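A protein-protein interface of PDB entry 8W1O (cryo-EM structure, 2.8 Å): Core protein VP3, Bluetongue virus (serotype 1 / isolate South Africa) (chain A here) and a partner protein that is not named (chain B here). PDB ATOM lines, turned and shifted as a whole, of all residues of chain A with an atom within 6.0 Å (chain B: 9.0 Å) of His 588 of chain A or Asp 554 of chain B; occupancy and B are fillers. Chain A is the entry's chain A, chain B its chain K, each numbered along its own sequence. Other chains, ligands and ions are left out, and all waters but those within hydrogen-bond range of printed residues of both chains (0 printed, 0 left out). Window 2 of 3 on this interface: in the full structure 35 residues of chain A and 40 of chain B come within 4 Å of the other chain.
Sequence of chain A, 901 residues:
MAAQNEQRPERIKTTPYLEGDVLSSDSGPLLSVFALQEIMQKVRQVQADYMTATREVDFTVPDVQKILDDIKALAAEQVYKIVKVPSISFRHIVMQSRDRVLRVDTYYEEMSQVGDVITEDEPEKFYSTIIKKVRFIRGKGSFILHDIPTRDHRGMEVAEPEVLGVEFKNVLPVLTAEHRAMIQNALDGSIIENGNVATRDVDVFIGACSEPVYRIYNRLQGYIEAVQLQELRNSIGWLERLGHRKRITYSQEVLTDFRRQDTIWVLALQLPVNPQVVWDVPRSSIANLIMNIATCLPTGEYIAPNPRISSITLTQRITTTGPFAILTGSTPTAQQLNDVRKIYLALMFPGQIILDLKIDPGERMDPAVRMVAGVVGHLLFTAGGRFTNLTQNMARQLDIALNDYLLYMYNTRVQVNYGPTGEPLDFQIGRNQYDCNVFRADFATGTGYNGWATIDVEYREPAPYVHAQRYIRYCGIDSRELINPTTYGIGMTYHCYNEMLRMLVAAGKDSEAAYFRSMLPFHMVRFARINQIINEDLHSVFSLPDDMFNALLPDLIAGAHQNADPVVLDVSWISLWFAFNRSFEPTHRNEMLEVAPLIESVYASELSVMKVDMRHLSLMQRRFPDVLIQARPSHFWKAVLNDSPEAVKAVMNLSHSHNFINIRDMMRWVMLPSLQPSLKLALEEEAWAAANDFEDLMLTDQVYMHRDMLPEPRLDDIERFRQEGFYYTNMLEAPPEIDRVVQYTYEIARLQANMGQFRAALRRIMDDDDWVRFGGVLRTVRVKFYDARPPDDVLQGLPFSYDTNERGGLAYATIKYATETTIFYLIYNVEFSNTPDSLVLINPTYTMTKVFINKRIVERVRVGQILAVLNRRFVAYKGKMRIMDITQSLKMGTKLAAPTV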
ATOM      1  N   LEU A 297      -0.648 -15.350 -26.832  1.00  0.00           N
ATOM      2  CA  LEU A 297      -0.703 -15.306 -25.370  1.00  0.00           C
ATOM      3  C   LEU A 297      -0.318 -13.921 -24.856  1.00  0.00           C
ATOM      4  O   LEU A 297       0.739 -13.403 -25.223  1.00  0.00           O
ATOM      5  CB  LEU A 297       0.214 -16.360 -24.763  1.00  0.00           C
ATOM      6  CG  LEU A 297      -0.059 -16.691 -23.294  1.00  0.00           C
ATOM      7  CD1 LEU A 297      -1.402 -17.378 -23.143  1.00  0.00           C
ATOM      8  CD2 LEU A 297       1.051 -17.549 -22.714  1.00  0.00           C
ATOM      9  N   PRO A 298      -1.144 -13.298 -24.002  1.00  0.00           N
ATOM     10  CA  PRO A 298      -0.783 -11.990 -23.438  1.00  0.00           C
ATOM     11  C   PRO A 298       0.056 -12.091 -22.173  1.00  0.00           C
ATOM     12  O   PRO A 298       0.332 -13.191 -21.688  1.00  0.00           O
ATOM     13  CB  PRO A 298      -2.149 -11.361 -23.147  1.00  0.00           C
ATOM     14  CG  PRO A 298      -2.998 -12.533 -22.792  1.00  0.00           C
ATOM     15  CD  PRO A 298      -2.522 -13.683 -23.650  1.00  0.00           C
ATOM     16  N   THR A 299       0.464 -10.944 -21.630  1.00  0.00           N
ATOM     17  CA  THR A 299       1.245 -10.882 -20.403  1.00  0.00           C
ATOM     18  C   THR A 299       0.543  -9.981 -19.397  1.00  0.00           C
ATOM     19  O   THR A 299      -0.179  -9.054 -19.772  1.00  0.00           O
ATOM     20  CB  THR A 299       2.666 -10.358 -20.655  1.00  0.00           C
ATOM     21  OG1 THR A 299       2.599  -9.059 -21.253  1.00  0.00           O
ATOM     22  CG2 THR A 299       3.428 -11.295 -21.575  1.00  0.00           C
ATOM     23  N   GLY A 300       0.759 -10.257 -18.120  1.00  0.00           N
ATOM     24  CA  GLY A 300       0.083  -9.496 -17.094  1.00  0.00           C
ATOM     25  C   GLY A 300       0.640  -9.751 -15.713  1.00  0.00           C
ATOM     26  O   GLY A 300       1.744 -10.272 -15.555  1.00  0.00           O
ATOM     27  N   PRO A 586      -4.234  -9.311 -17.208  1.00  0.00           N
ATOM     28  CA  PRO A 586      -3.385  -8.981 -18.362  1.00  0.00           C
ATOM     29  C   PRO A 586      -3.175  -7.478 -18.493  1.00  0.00           C
ATOM     30  O   PRO A 586      -4.127  -6.697 -18.441  1.00  0.00           O
ATOM     31  CB  PRO A 586      -4.168  -9.545 -19.552  1.00  0.00           C
ATOM     32  CG  PRO A 586      -5.577  -9.618 -19.078  1.00  0.00           C
ATOM     33  CD  PRO A 586      -5.509  -9.921 -17.614  1.00  0.00           C
ATOM     34  N   THR A 587      -1.916  -7.081 -18.671  1.00  0.00           N
ATOM     35  CA  THR A 587      -1.563  -5.680 -18.841  1.00  0.00           C
ATOM     36  C   THR A 587      -1.010  -5.354 -20.219  1.00  0.00           C
ATOM     37  O   THR A 587      -0.866  -4.171 -20.544  1.00  0.00           O
ATOM     38  CB  THR A 587      -0.532  -5.252 -17.783  1.00  0.00           C
ATOM     39  OG1 THR A 587       0.664  -6.022 -17.935  1.00  0.00           O
ATOM     40  CG2 THR A 587      -1.086  -5.459 -16.383  1.00  0.00           C
ATOM     41  N   HIS A 588      -0.699  -6.357 -21.036  1.00  0.00           N
ATOM     42  CA  HIS A 588      -0.048  -6.119 -22.322  1.00  0.00           C
ATOM     43  C   HIS A 588      -0.434  -7.251 -23.264  1.00  0.00           C
ATOM     44  O   HIS A 588      -0.058  -8.403 -23.037  1.00  0.00           O
ATOM     45  CB  HIS A 588       1.467  -6.020 -22.146  1.00  0.00           C
ATOM     46  CG  HIS A 588       2.251  -6.260 -23.400  1.00  0.00           C
ATOM     47  ND1 HIS A 588       2.723  -5.231 -24.187  1.00  0.00           N
ATOM     48  CD2 HIS A 588       2.684  -7.404 -23.980  1.00  0.00           C
ATOM     49  CE1 HIS A 588       3.387  -5.732 -25.212  1.00  0.00           C
ATOM     50  NE2 HIS A 588       3.380  -7.049 -25.109  1.00  0.00           N
ATOM     51  N   ARG A 589      -1.194  -6.925 -24.306  1.00  0.00           N
ATOM     52  CA  ARG A 589      -1.555  -7.915 -25.310  1.00  0.00           C
ATOM     53  C   ARG A 589      -0.353  -8.244 -26.190  1.00  0.00           C
ATOM     54  O   ARG A 589       0.589  -7.458 -26.310  1.00  0.00           O
ATOM     55  CB  ARG A 589      -2.722  -7.412 -26.160  1.00  0.00           C
ATOM     56  CG  ARG A 589      -3.996  -7.171 -25.368  1.00  0.00           C
ATOM     57  CD  ARG A 589      -5.134  -6.679 -26.249  1.00  0.00           C
ATOM     58  NE  ARG A 589      -6.046  -7.750 -26.631  1.00  0.00           N
ATOM     59  CZ  ARG A 589      -6.933  -7.662 -27.613  1.00  0.00           C
ATOM     60  NH1 ARG A 589      -7.061  -6.561 -28.333  1.00  0.00           N
ATOM     61  NH2 ARG A 589      -7.714  -8.706 -27.879  1.00  0.00           N
ATOM     62  N   ASN A 590      -0.391  -9.429 -26.799  1.00  0.00           N
ATOM     63  CA  ASN A 590       0.726  -9.901 -27.610  1.00  0.00           C
ATOM     64  C   ASN A 590       0.947  -8.993 -28.815  1.00  0.00           C
ATOM     65  O   ASN A 590      -0.003  -8.575 -29.481  1.00  0.00           O
ATOM     66  CB  ASN A 590       0.468 -11.337 -28.068  1.00  0.00           C
ATOM     67  CG  ASN A 590       1.722 -12.027 -28.562  1.00  0.00           C
ATOM     68  OD1 ASN A 590       2.242 -11.707 -29.629  1.00  0.00           O
ATOM     69  ND2 ASN A 590       2.214 -12.985 -27.789  1.00  0.00           N
ATOM     70  N   GLU A 591       2.215  -8.690 -29.096  1.00  0.00           N
ATOM     71  CA  GLU A 591       2.551  -7.761 -30.167  1.00  0.00           C
ATOM     72  C   GLU A 591       2.408  -8.364 -31.558  1.00  0.00           C
ATOM     73  O   GLU A 591       2.498  -7.625 -32.544  1.00  0.00           O
ATOM     74  CB  GLU A 591       3.978  -7.228 -29.989  1.00  0.00           C
ATOM     75  CG  GLU A 591       5.086  -8.248 -30.207  1.00  0.00           C
ATOM     76  CD  GLU A 591       5.391  -9.068 -28.967  1.00  0.00           C
ATOM     77  OE1 GLU A 591       4.569  -9.072 -28.026  1.00  0.00           O
ATOM     78  OE2 GLU A 591       6.459  -9.713 -28.936  1.00  0.00           O
ATOM     79  N   LYS A 895      -4.573  -2.460 -31.428  1.00  0.00           N
ATOM     80  CA  LYS A 895      -5.247  -3.266 -30.420  1.00  0.00           C
ATOM     81  C   LYS A 895      -5.962  -2.371 -29.417  1.00  0.00           C
ATOM     82  O   LYS A 895      -5.437  -1.337 -29.000  1.00  0.00           O
ATOM     83  CB  LYS A 895      -4.246  -4.166 -29.695  1.00  0.00           C
ATOM     84  CG  LYS A 895      -3.514  -5.140 -30.596  1.00  0.00           C
ATOM     85  CD  LYS A 895      -2.646  -6.096 -29.796  1.00  0.00           C
ATOM     86  CE  LYS A 895      -1.467  -5.381 -29.164  1.00  0.00           C
ATOM     87  NZ  LYS A 895      -0.571  -4.778 -30.183  1.00  0.00           N
ATOM     88  N   ASP B 288       6.223 -11.954 -15.486  1.00  0.00           N
ATOM     89  CA  ASP B 288       6.047 -11.435 -16.840  1.00  0.00           C
ATOM     90  C   ASP B 288       6.712 -10.074 -17.010  1.00  0.00           C
ATOM     91  O   ASP B 288       7.320  -9.799 -18.050  1.00  0.00           O
ATOM     92  CB  ASP B 288       4.559 -11.351 -17.180  1.00  0.00           C
ATOM     93  CG  ASP B 288       3.971 -12.696 -17.559  1.00  0.00           C
ATOM     94  OD1 ASP B 288       4.687 -13.711 -17.448  1.00  0.00           O
ATOM     95  OD2 ASP B 288       2.793 -12.739 -17.968  1.00  0.00           O
ATOM     96  N   ASP B 289       6.594  -9.207 -16.007  1.00  0.00           N
ATOM     97  CA  ASP B 289       7.237  -7.901 -16.069  1.00  0.00           C
ATOM     98  C   ASP B 289       8.752  -8.056 -16.021  1.00  0.00           C
ATOM     99  O   ASP B 289       9.286  -8.870 -15.263  1.00  0.00           O
ATOM    100  CB  ASP B 289       6.750  -7.021 -14.916  1.00  0.00           C
ATOM    101  CG  ASP B 289       7.182  -5.575 -15.060  1.00  0.00           C
ATOM    102  OD1 ASP B 289       8.332  -5.259 -14.699  1.00  0.00           O
ATOM    103  OD2 ASP B 289       6.371  -4.752 -15.533  1.00  0.00           O
ATOM    104  N   ILE B 550       4.495  -1.265 -12.364  1.00  0.00           N
ATOM    105  CA  ILE B 550       4.537  -1.845 -13.701  1.00  0.00           C
ATOM    106  C   ILE B 550       5.243  -0.876 -14.636  1.00  0.00           C
ATOM    107  O   ILE B 550       4.875   0.300 -14.729  1.00  0.00           O
ATOM    108  CB  ILE B 550       3.115  -2.170 -14.197  1.00  0.00           C
ATOM    109  CG1 ILE B 550       2.450  -3.199 -13.278  1.00  0.00           C
ATOM    110  CG2 ILE B 550       3.149  -2.680 -15.625  1.00  0.00           C
ATOM    111  CD1 ILE B 550       0.948  -3.063 -13.193  1.00  0.00           C
ATOM    112  N   THR B 551       6.263  -1.371 -15.338  1.00  0.00           N
ATOM    113  CA  THR B 551       7.075  -0.544 -16.224  1.00  0.00           C
ATOM    114  C   THR B 551       6.761  -0.769 -17.698  1.00  0.00           C
ATOM    115  O   THR B 551       7.547  -0.348 -18.556  1.00  0.00           O
ATOM    116  CB  THR B 551       8.565  -0.791 -15.969  1.00  0.00           C
ATOM    117  OG1 THR B 551       8.930  -2.082 -16.472  1.00  0.00           O
ATOM    118  CG2 THR B 551       8.869  -0.732 -14.482  1.00  0.00           C
ATOM    119  N   SER B 552       5.652  -1.423 -18.016  1.00  0.00           N
ATOM    120  CA  SER B 552       5.268  -1.619 -19.410  1.00  0.00           C
ATOM    121  C   SER B 552       4.869  -0.285 -20.034  1.00  0.00           C
ATOM    122  O   SER B 552       4.146   0.495 -19.405  1.00  0.00           O
ATOM    123  CB  SER B 552       4.114  -2.612 -19.512  1.00  0.00           C
ATOM    124  OG  SER B 552       3.572  -2.634 -20.820  1.00  0.00           O
ATOM    125  N   PRO B 553       5.325   0.018 -21.253  1.00  0.00           N
ATOM    126  CA  PRO B 553       4.928   1.285 -21.890  1.00  0.00           C
ATOM    127  C   PRO B 553       3.435   1.405 -22.139  1.00  0.00           C
ATOM    128  O   PRO B 553       2.920   2.525 -22.229  1.00  0.00           O
ATOM    129  CB  PRO B 553       5.723   1.274 -23.202  1.00  0.00           C
ATOM    130  CG  PRO B 553       6.885   0.381 -22.927  1.00  0.00           C
ATOM    131  CD  PRO B 553       6.342  -0.696 -22.040  1.00  0.00           C
ATOM    132  N   ASP B 554       2.721   0.283 -22.253  1.00  0.00           N
ATOM    133  CA  ASP B 554       1.278   0.321 -22.450  1.00  0.00           C
ATOM    134  C   ASP B 554       0.512   0.667 -21.180  1.00  0.00           C
ATOM    135  O   ASP B 554      -0.692   0.927 -21.259  1.00  0.00           O
ATOM    136  CB  ASP B 554       0.786  -1.023 -22.988  1.00  0.00           C
ATOM    137  CG  ASP B 554       0.941  -1.142 -24.489  1.00  0.00           C
ATOM    138  OD1 ASP B 554       1.214  -0.114 -25.143  1.00  0.00           O
ATOM    139  OD2 ASP B 554       0.785  -2.264 -25.014  1.00  0.00           O
ATOM    140  N   TYR B 555       1.169   0.669 -20.023  1.00  0.00           N
ATOM    141  CA  TYR B 555       0.496   0.976 -18.770  1.00  0.00           C
ATOM    142  C   TYR B 555       0.343   2.482 -18.607  1.00  0.00           C
ATOM    143  O   TYR B 555       1.259   3.252 -18.911  1.00  0.00           O
ATOM    144  CB  TYR B 555       1.272   0.390 -17.592  1.00  0.00           C
ATOM    145  CG  TYR B 555       0.443   0.218 -16.344  1.00  0.00           C
ATOM    146  CD1 TYR B 555      -0.567  -0.733 -16.287  1.00  0.00           C
ATOM    147  CD2 TYR B 555       0.665   1.007 -15.226  1.00  0.00           C
ATOM    148  CE1 TYR B 555      -1.329  -0.896 -15.147  1.00  0.00           C
ATOM    149  CE2 TYR B 555      -0.092   0.853 -14.082  1.00  0.00           C
ATOM    150  CZ  TYR B 555      -1.088  -0.100 -14.048  1.00  0.00           C
ATOM    151  OH  TYR B 555      -1.846  -0.259 -12.911  1.00  0.00           O
ATOM    152  N   LYS B 556      -0.828   2.900 -18.122  1.00  0.00           N
ATOM    153  CA  LYS B 556      -1.158   4.322 -18.090  1.00  0.00           C
ATOM    154  C   LYS B 556      -0.367   5.066 -17.019  1.00  0.00           C
ATOM    155  O   LYS B 556       0.167   6.151 -17.273  1.00  0.00           O
ATOM    156  CB  LYS B 556      -2.659   4.507 -17.878  1.00  0.00           C
ATOM    157  CG  LYS B 556      -3.094   5.960 -17.873  1.00  0.00           C
ATOM    158  CD  LYS B 556      -2.834   6.625 -19.216  1.00  0.00           C
ATOM    159  CE  LYS B 556      -3.752   6.092 -20.301  1.00  0.00           C
ATOM    160  NZ  LYS B 556      -3.525   6.798 -21.592  1.00  0.00           N
ATOM    161  N   LYS B 557      -0.288   4.504 -15.818  1.00  0.00           N
ATOM    162  CA  LYS B 557       0.314   5.208 -14.697  1.00  0.00           C
ATOM    163  C   LYS B 557       1.830   5.290 -14.847  1.00  0.00           C
ATOM    164  O   LYS B 557       2.475   4.388 -15.388  1.00  0.00           O
ATOM    165  CB  LYS B 557      -0.055   4.520 -13.384  1.00  0.00           C
ATOM    166  CG  LYS B 557      -1.531   4.635 -13.046  1.00  0.00           C
ATOM    167  CD  LYS B 557      -1.867   3.969 -11.726  1.00  0.00           C
ATOM    168  CE  LYS B 557      -3.354   4.083 -11.427  1.00  0.00           C
ATOM    169  NZ  LYS B 557      -3.723   3.429 -10.143  1.00  0.00           N
ATOM    170  N   LYS B 561       7.348   3.790 -13.630  1.00  0.00           N
ATOM    171  CA  LYS B 561       8.466   4.092 -14.518  1.00  0.00           C
ATOM    172  C   LYS B 561       9.603   4.780 -13.774  1.00  0.00           C
ATOM    173  O   LYS B 561      10.777   4.521 -14.055  1.00  0.00           O
ATOM    174  CB  LYS B 561       7.993   4.960 -15.685  1.00  0.00           C
ATOM    175  CG  LYS B 561       6.632   4.582 -16.241  1.00  0.00           C
ATOM    176  CD  LYS B 561       6.651   3.199 -16.862  1.00  0.00           C
ATOM    177  CE  LYS B 561       5.264   2.783 -17.321  1.00  0.00           C
ATOM    178  NZ  LYS B 561       4.701   3.715 -18.334  1.00  0.00           N
ATOM    179  N   GLN B 743      10.726   7.002 -28.410  1.00  0.00           N
ATOM    180  CA  GLN B 743       9.880   5.890 -28.828  1.00  0.00           C
ATOM    181  C   GLN B 743       8.989   6.286 -29.997  1.00  0.00           C
ATOM    182  O   GLN B 743       8.854   5.534 -30.971  1.00  0.00           O
ATOM    183  CB  GLN B 743       9.033   5.408 -27.651  1.00  0.00           C
ATOM    184  CG  GLN B 743       9.726   4.411 -26.747  1.00  0.00           C
ATOM    185  CD  GLN B 743       9.073   4.316 -25.386  1.00  0.00           C
ATOM    186  OE1 GLN B 743       7.899   3.966 -25.271  1.00  0.00           O
ATOM    187  NE2 GLN B 743       9.831   4.631 -24.344  1.00  0.00           N
ATOM    188  N   THR B 755      10.182  -3.274 -30.620  1.00  0.00           N
ATOM    189  CA  THR B 755       9.066  -3.218 -29.688  1.00  0.00           C
ATOM    190  C   THR B 755       9.612  -3.008 -28.283  1.00  0.00           C
ATOM    191  O   THR B 755      10.609  -3.626 -27.897  1.00  0.00           O
ATOM    192  CB  THR B 755       8.198  -4.480 -29.770  1.00  0.00           C
ATOM    193  OG1 THR B 755       7.124  -4.393 -28.825  1.00  0.00           O
ATOM    194  CG2 THR B 755       9.004  -5.739 -29.510  1.00  0.00           C
ATOM    195  N   PHE B 756       8.980  -2.110 -27.536  1.00  0.00           N
ATOM    196  CA  PHE B 756       9.458  -1.724 -26.217  1.00  0.00           C
ATOM    197  C   PHE B 756       8.665  -2.455 -25.144  1.00  0.00           C
ATOM    198  O   PHE B 756       7.431  -2.412 -25.136  1.00  0.00           O
ATOM    199  CB  PHE B 756       9.345  -0.211 -26.029  1.00  0.00           C
ATOM    200  CG  PHE B 756      10.229   0.583 -26.951  1.00  0.00           C
ATOM    201  CD1 PHE B 756       9.805   0.914 -28.227  1.00  0.00           C
ATOM    202  CD2 PHE B 756      11.479   1.005 -26.537  1.00  0.00           C
ATOM    203  CE1 PHE B 756      10.616   1.642 -29.075  1.00  0.00           C
ATOM    204  CE2 PHE B 756      12.293   1.733 -27.378  1.00  0.00           C
ATOM    205  CZ  PHE B 756      11.861   2.052 -28.649  1.00  0.00           C
ATOM    206  N   LEU B 757       9.378  -3.130 -24.244  1.00  0.00           N
ATOM    207  CA  LEU B 757       8.760  -3.891 -23.166  1.00  0.00           C
ATOM    208  C   LEU B 757       8.882  -3.210 -21.811  1.00  0.00           C
ATOM    209  O   LEU B 757       8.045  -3.441 -20.934  1.00  0.00           O
ATOM    210  CB  LEU B 757       9.381  -5.290 -23.084  1.00  0.00           C
ATOM    211  CG  LEU B 757       9.300  -6.167 -24.334  1.00  0.00           C
ATOM    212  CD1 LEU B 757      10.120  -7.430 -24.147  1.00  0.00           C
ATOM    213  CD2 LEU B 757       7.857  -6.511 -24.657  1.00  0.00           C
ATOM    214  N   SER B 758       9.903  -2.381 -21.614  1.00  0.00           N
ATOM    215  CA  SER B 758      10.140  -1.755 -20.323  1.00  0.00           C
ATOM    216  C   SER B 758      10.856  -0.428 -20.523  1.00  0.00           C
ATOM    217  O   SER B 758      11.710  -0.303 -21.403  1.00  0.00           O
ATOM    218  CB  SER B 758      10.966  -2.668 -19.410  1.00  0.00           C
ATOM    219  OG  SER B 758      11.220  -2.056 -18.158  1.00  0.00           O
ATOM    220  N   GLU B 759      10.498   0.558 -19.702  1.00  0.00           N
ATOM    221  CA  GLU B 759      11.160   1.853 -19.681  1.00  0.00           C
ATOM    222  C   GLU B 759      11.395   2.272 -18.236  1.00  0.00           C
ATOM    223  O   GLU B 759      10.509   2.137 -17.387  1.00  0.00           O
ATOM    224  CB  GLU B 759      10.336   2.916 -20.427  1.00  0.00           C
ATOM    225  CG  GLU B 759       8.934   3.140 -19.882  1.00  0.00           C
ATOM    226  CD  GLU B 759       8.091   4.014 -20.782  1.00  0.00           C
ATOM    227  OE1 GLU B 759       8.661   4.883 -21.473  1.00  0.00           O
ATOM    228  OE2 GLU B 759       6.854   3.834 -20.798  1.00  0.00           O
ATOM    229  N   LYS B 771      12.765  -5.863 -27.779  1.00  0.00           N
ATOM    230  CA  LYS B 771      12.984  -7.002 -28.657  1.00  0.00           C
ATOM    231  C   LYS B 771      13.298  -6.489 -30.054  1.00  0.00           C
ATOM    232  O   LYS B 771      12.610  -5.603 -30.569  1.00  0.00           O
ATOM    233  CB  LYS B 771      11.762  -7.925 -28.709  1.00  0.00           C
ATOM    234  CG  LYS B 771      11.533  -8.745 -27.455  1.00  0.00           C
ATOM    235  CD  LYS B 771      10.140  -9.353 -27.446  1.00  0.00           C
ATOM    236  CE  LYS B 771      10.177 -10.826 -27.814  1.00  0.00           C
ATOM    237  NZ  LYS B 771       9.198 -11.619 -27.018  1.00  0.00           N
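The side-chain carboxylate (OE2) of Glu 591 of chain A is in salt-bridge range of the side-chain amino group (NZ) of Lys 771 of chain B (3.8 Å).
The side-chain carboxylate (OD2) of Asp 288 of chain B lies within hydrogen-bond range of the backbone NH (N) of Gly 300 of chain A, 3.2 Å away.
Of the 11 printed residues of chain A, 4 touch a printed residue of chain B.
Among the printed residues, Asp or Glu carboxylates within 4 Å of a Lys or Arg side-chain nitrogen of the other chain: Glu 591 of chain A with Lys 771 of chain B (3.8 Å).
The side-chain hydroxyl (OG) of Ser 552 of chain B lies close to the backbone NH (N) of Asp 554 of chain B (3.4 Å).
The backbone carbonyl oxygen (O) of Thr 299 of chain A is in hydrogen-bond range of the backbone NH (N) of Thr 587 of chain A (2.8 Å).
The backbone carbonyl oxygen of Thr 755 of chain B sits at hydrogen-bond distance from the backbone NH of Lys 771 of chain B, at 3.1 Å.
The backbone carbonyl oxygen of His 588 of chain A is in hydrogen-bond range of the backbone NH of Thr 299 of chain A.
Among the printed residues, pairs that only touch across the chains: Thr 299 of chain A with Asp 288 of chain B (3.4 Å) and His 588 of chain A with Asp 554 of chain B (3.6 Å).
His 588 of chain A touches one residue of chain B.
Of the printed residues of chain A, Asp 554 of chain B touches His 588 (3.6 Å).
Thr 299 of chain A touches just one residue of chain B: Asp 288.
No residue of chain B comes within 4 Å of Thr 587 of chain A.
Of the printed residues of chain B, Gly 300 of chain A touches Asp 288 (3.2 Å).
Of the printed residues of chain A, Lys 771 of chain B touches Glu 591 (3.8 Å).
Of the printed residues of chain B, Glu 591 of chain A touches Lys 771 (3.8 Å).
Asn 590 of chain A touches none of the printed residues of chain B.
Ser 758 of chain B touches none of the printed residues of chain A.
The nearest residue of chain B that does not touch His 588 of chain A is Ser 552 of chain B (4.2 Å).
The nearest residue of chain A that does not touch Asp 554 of chain B is Thr 587 of chain A (4.3 Å).
The nearest printed residue of chain B that does not touch Gly 300 of chain A is Asp 289 of chain B (5.0 Å).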
